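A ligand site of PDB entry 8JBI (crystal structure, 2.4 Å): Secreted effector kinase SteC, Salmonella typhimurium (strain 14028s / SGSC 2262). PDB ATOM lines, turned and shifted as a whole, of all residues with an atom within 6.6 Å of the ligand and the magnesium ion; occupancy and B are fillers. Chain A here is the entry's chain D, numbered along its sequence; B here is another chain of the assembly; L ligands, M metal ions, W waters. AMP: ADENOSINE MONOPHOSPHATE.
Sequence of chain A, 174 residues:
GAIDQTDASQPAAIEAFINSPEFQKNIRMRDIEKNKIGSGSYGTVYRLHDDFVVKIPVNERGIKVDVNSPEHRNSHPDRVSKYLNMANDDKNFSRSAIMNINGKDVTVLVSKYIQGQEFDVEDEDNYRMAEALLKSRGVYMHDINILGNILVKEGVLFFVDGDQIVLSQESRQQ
Water W1 lies within hydrogen-bond range of the backbone NH (N) of Asp 161 of chain B, a nitrogen (N7) of the ligand and the side-chain hydroxyl (OG) of Ser 111.
The backbone carbonyl oxygen of Ser 39 sits close to the side-chain hydroxyl of Tyr 42. The backbone NH (N) of Gly 40 lies close to the side-chain hydroxyl (OH) of Tyr 42 (3.5 Å). The backbone NH of Lys 112 is in hydrogen-bond range of the backbone carbonyl oxygen of Phe 93 (3.0 Å). O of Gly 38 is in hydrogen-bond range of N of Val 45 (3.1 Å). O of Val 160 of chain B sits at hydrogen-bond distance from N of Asn 149 of chain B (2.8 Å). The backbone carbonyl oxygen (O) of Val 45 lies within hydrogen-bond range of the backbone NH (N) of Ile 37. The backbone carbonyl oxygen of Ser 111 lies within hydrogen-bond range of the backbone NH of Val 53, at 2.9 Å.
No residue comes within 4 Å of the magnesium ion. The nearest printed residue that does not touch the magnesium ion is Asn 149 of chain B (4.7 Å).
O of Ser 39 sits close to O1P of the ligand (3.4 Å). Residues that only touch the ligand: Gly 38, Val 45, Val 53, Ser 111, Tyr 113 and Val 160 of chain B. Hydrophobic or aromatic side chains within 4 Å of the ligand: Tyr 42, Val 45, Val 53, Tyr 113, Ile 114 and Val 160 of chain B. The nearest printed residue that does not touch the ligand is Asp 161 of chain B (4.1 Å).
The magnesium ion is bound by an oxygen (O3P) of the ligand (1.8 Å).
OH of Tyr 42 is in hydrogen-bond range of O1P of the ligand, 2.6 Å away. O of Lys 112 is in hydrogen-bond range of N6 of the ligand. A nitrogen (N1) of the ligand lies within hydrogen-bond range of the backbone NH of Ile 114.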
ATOM      1  N   ILE A  37      14.119   8.007   4.397  1.00  0.00           N
ATOM      2  CA  ILE A  37      13.971   6.849   3.536  1.00  0.00           C
ATOM      3  C   ILE A  37      15.086   6.773   2.500  1.00  0.00           C
ATOM      4  O   ILE A  37      15.379   5.703   1.965  1.00  0.00           O
ATOM      5  CB  ILE A  37      12.613   6.852   2.816  1.00  0.00           C
ATOM      6  CG1 ILE A  37      12.481   8.080   1.928  1.00  0.00           C
ATOM      7  CG2 ILE A  37      11.483   6.815   3.822  1.00  0.00           C
ATOM      8  CD1 ILE A  37      11.157   8.183   1.219  1.00  0.00           C
ATOM      9  N   GLY A  38      15.703   7.915   2.226  1.00  0.00           N
ATOM     10  CA  GLY A  38      16.784   7.984   1.260  1.00  0.00           C
ATOM     11  C   GLY A  38      17.655   9.216   1.451  1.00  0.00           C
ATOM     12  O   GLY A  38      17.208  10.208   2.020  1.00  0.00           O
ATOM     13  N   SER A  39      18.889   9.133   0.974  1.00  0.00           N
ATOM     14  CA  SER A  39      19.843  10.244   1.057  1.00  0.00           C
ATOM     15  C   SER A  39      21.006  10.058   0.078  1.00  0.00           C
ATOM     16  O   SER A  39      21.417   8.936  -0.196  1.00  0.00           O
ATOM     17  CB  SER A  39      20.365  10.398   2.484  1.00  0.00           C
ATOM     18  OG  SER A  39      20.758   9.144   3.002  1.00  0.00           O
ATOM     19  N   GLY A  40      21.528  11.166  -0.438  1.00  0.00           N
ATOM     20  CA  GLY A  40      22.651  11.144  -1.355  1.00  0.00           C
ATOM     21  C   GLY A  40      23.237  12.532  -1.459  1.00  0.00           C
ATOM     22  O   GLY A  40      22.838  13.415  -0.703  1.00  0.00           O
ATOM     23  N   TYR A  42      22.782  14.818  -3.506  1.00  0.00           N
ATOM     24  CA  TYR A  42      21.716  15.749  -3.874  1.00  0.00           C
ATOM     25  C   TYR A  42      21.012  16.364  -2.671  1.00  0.00           C
ATOM     26  O   TYR A  42      20.704  17.566  -2.674  1.00  0.00           O
ATOM     27  CB  TYR A  42      20.698  15.012  -4.743  1.00  0.00           C
ATOM     28  CG  TYR A  42      20.321  13.630  -4.220  1.00  0.00           C
ATOM     29  CD1 TYR A  42      19.273  13.471  -3.322  1.00  0.00           C
ATOM     30  CD2 TYR A  42      21.019  12.497  -4.614  1.00  0.00           C
ATOM     31  CE1 TYR A  42      18.920  12.227  -2.836  1.00  0.00           C
ATOM     32  CE2 TYR A  42      20.679  11.246  -4.127  1.00  0.00           C
ATOM     33  CZ  TYR A  42      19.634  11.120  -3.231  1.00  0.00           C
ATOM     34  OH  TYR A  42      19.259   9.894  -2.737  1.00  0.00           O
ATOM     35  N   VAL A  45      15.525  12.728   1.410  1.00  0.00           N
ATOM     36  CA  VAL A  45      14.073  12.621   1.357  1.00  0.00           C
ATOM     37  C   VAL A  45      13.501  11.994   2.629  1.00  0.00           C
ATOM     38  O   VAL A  45      13.941  10.925   3.068  1.00  0.00           O
ATOM     39  CB  VAL A  45      13.615  11.863   0.099  1.00  0.00           C
ATOM     40  CG1 VAL A  45      14.318  10.541  -0.015  1.00  0.00           C
ATOM     41  CG2 VAL A  45      12.114  11.665   0.111  1.00  0.00           C
ATOM     42  N   VAL A  53       6.308  13.020   0.629  1.00  0.00           N
ATOM     43  CA  VAL A  53       7.700  13.056   1.013  1.00  0.00           C
ATOM     44  C   VAL A  53       8.258  14.451   0.759  1.00  0.00           C
ATOM     45  O   VAL A  53       7.707  15.225  -0.036  1.00  0.00           O
ATOM     46  CB  VAL A  53       8.555  11.988   0.286  1.00  0.00           C
ATOM     47  CG1 VAL A  53       7.877  10.636   0.347  1.00  0.00           C
ATOM     48  CG2 VAL A  53       8.786  12.394  -1.147  1.00  0.00           C
ATOM     49  N   PHE A  93       1.085  16.801  -8.291  1.00  0.00           N
ATOM     50  CA  PHE A  93       2.060  15.786  -7.898  1.00  0.00           C
ATOM     51  C   PHE A  93       3.143  16.334  -6.966  1.00  0.00           C
ATOM     52  O   PHE A  93       3.525  15.653  -6.006  1.00  0.00           O
ATOM     53  CB  PHE A  93       2.706  15.126  -9.117  1.00  0.00           C
ATOM     54  CG  PHE A  93       3.448  13.861  -8.772  1.00  0.00           C
ATOM     55  CD1 PHE A  93       2.759  12.675  -8.534  1.00  0.00           C
ATOM     56  CD2 PHE A  93       4.838  13.864  -8.679  1.00  0.00           C
ATOM     57  CE1 PHE A  93       3.434  11.506  -8.204  1.00  0.00           C
ATOM     58  CE2 PHE A  93       5.526  12.688  -8.349  1.00  0.00           C
ATOM     59  CZ  PHE A  93       4.815  11.507  -8.109  1.00  0.00           C
ATOM     60  N   SER A 111       6.653  15.948  -2.778  1.00  0.00           N
ATOM     61  CA  SER A 111       5.969  15.097  -3.756  1.00  0.00           C
ATOM     62  C   SER A 111       5.005  14.115  -3.095  1.00  0.00           C
ATOM     63  O   SER A 111       5.143  13.814  -1.905  1.00  0.00           O
ATOM     64  CB  SER A 111       6.974  14.316  -4.608  1.00  0.00           C
ATOM     65  OG  SER A 111       8.162  15.052  -4.831  1.00  0.00           O
ATOM     66  N   LYS A 112       4.047  13.617  -3.860  1.00  0.00           N
ATOM     67  CA  LYS A 112       3.209  12.510  -3.389  1.00  0.00           C
ATOM     68  C   LYS A 112       4.106  11.327  -3.069  1.00  0.00           C
ATOM     69  O   LYS A 112       5.065  11.040  -3.812  1.00  0.00           O
ATOM     70  CB  LYS A 112       2.174  12.131  -4.448  1.00  0.00           C
ATOM     71  CG  LYS A 112       1.138  13.211  -4.694  1.00  0.00           C
ATOM     72  CD  LYS A 112       0.013  12.761  -5.624  1.00  0.00           C
ATOM     73  CE  LYS A 112      -1.080  13.842  -5.720  1.00  0.00           C
ATOM     74  NZ  LYS A 112      -2.028  13.620  -6.844  1.00  0.00           N
ATOM     75  N   TYR A 113       3.832  10.663  -1.941  1.00  0.00           N
ATOM     76  CA  TYR A 113       4.581   9.451  -1.607  1.00  0.00           C
ATOM     77  C   TYR A 113       4.025   8.314  -2.441  1.00  0.00           C
ATOM     78  O   TYR A 113       2.817   8.107  -2.485  1.00  0.00           O
ATOM     79  CB  TYR A 113       4.474   9.124  -0.117  1.00  0.00           C
ATOM     80  CG  TYR A 113       5.015   7.752   0.217  1.00  0.00           C
ATOM     81  CD1 TYR A 113       6.384   7.476   0.117  1.00  0.00           C
ATOM     82  CD2 TYR A 113       4.171   6.724   0.604  1.00  0.00           C
ATOM     83  CE1 TYR A 113       6.890   6.222   0.410  1.00  0.00           C
ATOM     84  CE2 TYR A 113       4.659   5.454   0.895  1.00  0.00           C
ATOM     85  CZ  TYR A 113       6.020   5.221   0.802  1.00  0.00           C
ATOM     86  OH  TYR A 113       6.515   3.962   1.088  1.00  0.00           O
ATOM     87  N   ILE A 114       4.907   7.604  -3.138  1.00  0.00           N
ATOM     88  CA  ILE A 114       4.460   6.474  -3.950  1.00  0.00           C
ATOM     89  C   ILE A 114       5.047   5.190  -3.398  1.00  0.00           C
ATOM     90  O   ILE A 114       6.262   4.975  -3.473  1.00  0.00           O
ATOM     91  CB  ILE A 114       4.882   6.584  -5.419  1.00  0.00           C
ATOM     92  CG1 ILE A 114       4.415   7.912  -6.041  1.00  0.00           C
ATOM     93  CG2 ILE A 114       4.337   5.400  -6.205  1.00  0.00           C
ATOM     94  CD1 ILE A 114       2.894   8.063  -6.150  1.00  0.00           C
ATOM     95  N   GLN A 115       4.184   4.342  -2.849  1.00  0.00           N
ATOM     96  CA  GLN A 115       4.628   3.044  -2.377  1.00  0.00           C
ATOM     97  C   GLN A 115       4.537   2.066  -3.534  1.00  0.00           C
ATOM     98  O   GLN A 115       3.452   1.655  -3.932  1.00  0.00           O
ATOM     99  CB  GLN A 115       3.777   2.575  -1.206  1.00  0.00           C
ATOM    100  CG  GLN A 115       4.498   1.617  -0.261  1.00  0.00           C
ATOM    101  CD  GLN A 115       3.574   0.980   0.770  1.00  0.00           C
ATOM    102  OE1 GLN A 115       2.383   1.291   0.815  1.00  0.00           O
ATOM    103  NE2 GLN A 115       4.123   0.080   1.581  1.00  0.00           N
ATOM    104  N   GLY A 116       5.678   1.689  -4.088  1.00  0.00           N
ATOM    105  CA  GLY A 116       5.706   0.753  -5.195  1.00  0.00           C
ATOM    106  C   GLY A 116       7.075   0.147  -5.362  1.00  0.00           C
ATOM    107  O   GLY A 116       8.012   0.466  -4.622  1.00  0.00           O
ATOM    108  N   GLU A 118      10.463  -0.786  -7.931  1.00  0.00           N
ATOM    109  CA  GLU A 118      11.149  -0.174  -9.053  1.00  0.00           C
ATOM    110  C   GLU A 118      10.660  -0.819 -10.339  1.00  0.00           C
ATOM    111  O   GLU A 118      10.610  -2.055 -10.448  1.00  0.00           O
ATOM    112  CB  GLU A 118      12.668  -0.328  -8.953  1.00  0.00           C
ATOM    113  CG  GLU A 118      13.397   0.342 -10.105  1.00  0.00           C
ATOM    114  CD  GLU A 118      14.641   1.100  -9.662  1.00  0.00           C
ATOM    115  OE1 GLU A 118      14.654   2.347  -9.778  1.00  0.00           O
ATOM    116  OE2 GLU A 118      15.606   0.439  -9.219  1.00  0.00           O
ATOM    117  N   ASN B 149      13.217   8.641 -11.566  1.00  0.00           N
ATOM    118  CA  ASN B 149      13.112   7.193 -11.443  1.00  0.00           C
ATOM    119  C   ASN B 149      11.688   6.714 -11.780  1.00  0.00           C
ATOM    120  O   ASN B 149      10.734   7.488 -11.704  1.00  0.00           O
ATOM    121  CB  ASN B 149      13.539   6.720 -10.040  1.00  0.00           C
ATOM    122  CG  ASN B 149      15.040   6.935  -9.743  1.00  0.00           C
ATOM    123  OD1 ASN B 149      15.860   7.110 -10.653  1.00  0.00           O
ATOM    124  ND2 ASN B 149      15.397   6.906  -8.457  1.00  0.00           N
ATOM    125  N   LEU B 151       8.567   4.200 -10.818  1.00  0.00           N
ATOM    126  CA  LEU B 151       7.933   3.295  -9.862  1.00  0.00           C
ATOM    127  C   LEU B 151       6.617   2.780 -10.431  1.00  0.00           C
ATOM    128  O   LEU B 151       5.918   3.487 -11.164  1.00  0.00           O
ATOM    129  CB  LEU B 151       7.663   3.993  -8.535  1.00  0.00           C
ATOM    130  CG  LEU B 151       8.863   4.671  -7.870  1.00  0.00           C
ATOM    131  CD1 LEU B 151       8.411   5.453  -6.654  1.00  0.00           C
ATOM    132  CD2 LEU B 151       9.915   3.634  -7.480  1.00  0.00           C
ATOM    133  N   PHE B 159       6.390   8.735 -11.746  1.00  0.00           N
ATOM    134  CA  PHE B 159       7.697   9.286 -12.069  1.00  0.00           C
ATOM    135  C   PHE B 159       8.138  10.186 -10.928  1.00  0.00           C
ATOM    136  O   PHE B 159       7.467  11.162 -10.598  1.00  0.00           O
ATOM    137  CB  PHE B 159       7.590  10.021 -13.400  1.00  0.00           C
ATOM    138  CG  PHE B 159       7.189   9.107 -14.520  1.00  0.00           C
ATOM    139  CD1 PHE B 159       8.123   8.272 -15.112  1.00  0.00           C
ATOM    140  CD2 PHE B 159       5.867   9.030 -14.954  1.00  0.00           C
ATOM    141  CE1 PHE B 159       7.772   7.382 -16.141  1.00  0.00           C
ATOM    142  CE2 PHE B 159       5.490   8.166 -15.978  1.00  0.00           C
ATOM    143  CZ  PHE B 159       6.448   7.317 -16.568  1.00  0.00           C
ATOM    144  N   VAL B 160       9.232   9.810 -10.271  1.00  0.00           N
ATOM    145  CA  VAL B 160       9.698  10.531  -9.097  1.00  0.00           C
ATOM    146  C   VAL B 160      11.103  11.061  -9.341  1.00  0.00           C
ATOM    147  O   VAL B 160      11.769  10.632 -10.284  1.00  0.00           O
ATOM    148  CB  VAL B 160       9.674   9.636  -7.835  1.00  0.00           C
ATOM    149  CG1 VAL B 160       8.245   9.276  -7.457  1.00  0.00           C
ATOM    150  CG2 VAL B 160      10.467   8.359  -8.058  1.00  0.00           C
ATOM    151  N   ASP B 161      11.524  11.995  -8.504  1.00  0.00           N
ATOM    152  CA  ASP B 161      12.871  12.538  -8.591  1.00  0.00           C
ATOM    153  C   ASP B 161      13.869  11.402  -8.415  1.00  0.00           C
ATOM    154  O   ASP B 161      13.752  10.590  -7.505  1.00  0.00           O
ATOM    155  CB  ASP B 161      13.057  13.588  -7.499  1.00  0.00           C
ATOM    156  CG  ASP B 161      14.421  14.235  -7.554  1.00  0.00           C
ATOM    157  OD1 ASP B 161      14.914  14.515  -8.678  1.00  0.00           O
ATOM    158  OD2 ASP B 161      14.986  14.469  -6.479  1.00  0.00           O
ATOM    159  N   GLY B 162      14.835  11.333  -9.330  1.00  0.00           N
ATOM    160  CA  GLY B 162      15.763  10.211  -9.343  1.00  0.00           C
ATOM    161  C   GLY B 162      16.882  10.427 -10.329  1.00  0.00           C
ATOM    162  O   GLY B 162      17.243  11.566 -10.614  1.00  0.00           O
ATOM    163  N   ASP B 163      17.443   9.339 -10.858  1.00  0.00           N
ATOM    164  CA  ASP B 163      18.551   9.471 -11.789  1.00  0.00           C
ATOM    165  C   ASP B 163      18.727   8.298 -12.753  1.00  0.00           C
ATOM    166  O   ASP B 163      19.854   7.983 -13.144  1.00  0.00           O
ATOM    167  CB  ASP B 163      19.855   9.719 -11.028  1.00  0.00           C
ATOM    168  CG  ASP B 163      20.201   8.602 -10.033  1.00  0.00           C
ATOM    169  OD1 ASP B 163      19.628   7.485 -10.113  1.00  0.00           O
ATOM    170  OD2 ASP B 163      21.088   8.845  -9.179  1.00  0.00           O
ATOM    171  N   GLN B 164      17.637   7.679 -13.178  1.00  0.00           N
ATOM    172  CA  GLN B 164      17.755   6.487 -14.016  1.00  0.00           C
ATOM    173  C   GLN B 164      17.342   6.685 -15.468  1.00  0.00           C
ATOM    174  O   GLN B 164      17.745   5.922 -16.357  1.00  0.00           O
ATOM    175  CB  GLN B 164      17.003   5.305 -13.389  1.00  0.00           C
ATOM    176  CG  GLN B 164      17.529   4.885 -12.011  1.00  0.00           C
ATOM    177  CD  GLN B 164      18.945   4.276 -12.033  1.00  0.00           C
ATOM    178  OE1 GLN B 164      19.636   4.288 -13.054  1.00  0.00           O
ATOM    179  NE2 GLN B 164      19.363   3.746 -10.888  1.00  0.00           N
HETATM  180  P   AMP L   1      18.231   7.097  -3.239  1.00  0.00           P
HETATM  181  O1P AMP L   1      19.527   7.327  -2.524  1.00  0.00           O
HETATM  182  O2P AMP L   1      17.959   8.107  -4.324  1.00  0.00           O
HETATM  183  O3P AMP L   1      18.067   5.671  -3.712  1.00  0.00           O
HETATM  184  O5' AMP L   1      17.086   7.341  -2.134  1.00  0.00           O
HETATM  185  C5' AMP L   1      15.870   8.027  -2.512  1.00  0.00           C
HETATM  186  C4' AMP L   1      14.713   7.071  -2.350  1.00  0.00           C
HETATM  187  O4' AMP L   1      13.469   7.817  -2.237  1.00  0.00           O
HETATM  188  C3' AMP L   1      14.498   6.080  -3.504  1.00  0.00           C
HETATM  189  O3' AMP L   1      14.147   4.798  -3.003  1.00  0.00           O
HETATM  190  C2' AMP L   1      13.342   6.717  -4.275  1.00  0.00           C
HETATM  191  O2' AMP L   1      12.618   5.790  -5.054  1.00  0.00           O
HETATM  192  C1' AMP L   1      12.519   7.253  -3.108  1.00  0.00           C
HETATM  193  N9  AMP L   1      11.558   8.264  -3.492  1.00  0.00           N
HETATM  194  C8  AMP L   1      11.829   9.503  -4.018  1.00  0.00           C
HETATM  195  N7  AMP L   1      10.755  10.210  -4.265  1.00  0.00           N
HETATM  196  C5  AMP L   1       9.703   9.387  -3.868  1.00  0.00           C
HETATM  197  C6  AMP L   1       8.306   9.563  -3.877  1.00  0.00           C
HETATM  198  N6  AMP L   1       7.705  10.667  -4.303  1.00  0.00           N
HETATM  199  N1  AMP L   1       7.552   8.541  -3.421  1.00  0.00           N
HETATM  200  C2  AMP L   1       8.167   7.434  -2.986  1.00  0.00           C
HETATM  201  N3  AMP L   1       9.460   7.155  -2.930  1.00  0.00           N
HETATM  202  C4  AMP L   1      10.188   8.188  -3.397  1.00  0.00           C
HETATM  203 MG    MG M   1      18.602   5.278  -5.407  1.00  0.00          MG
HETATM  204  O   HOH W   1       9.852  12.375  -6.147  1.00  0.00           O
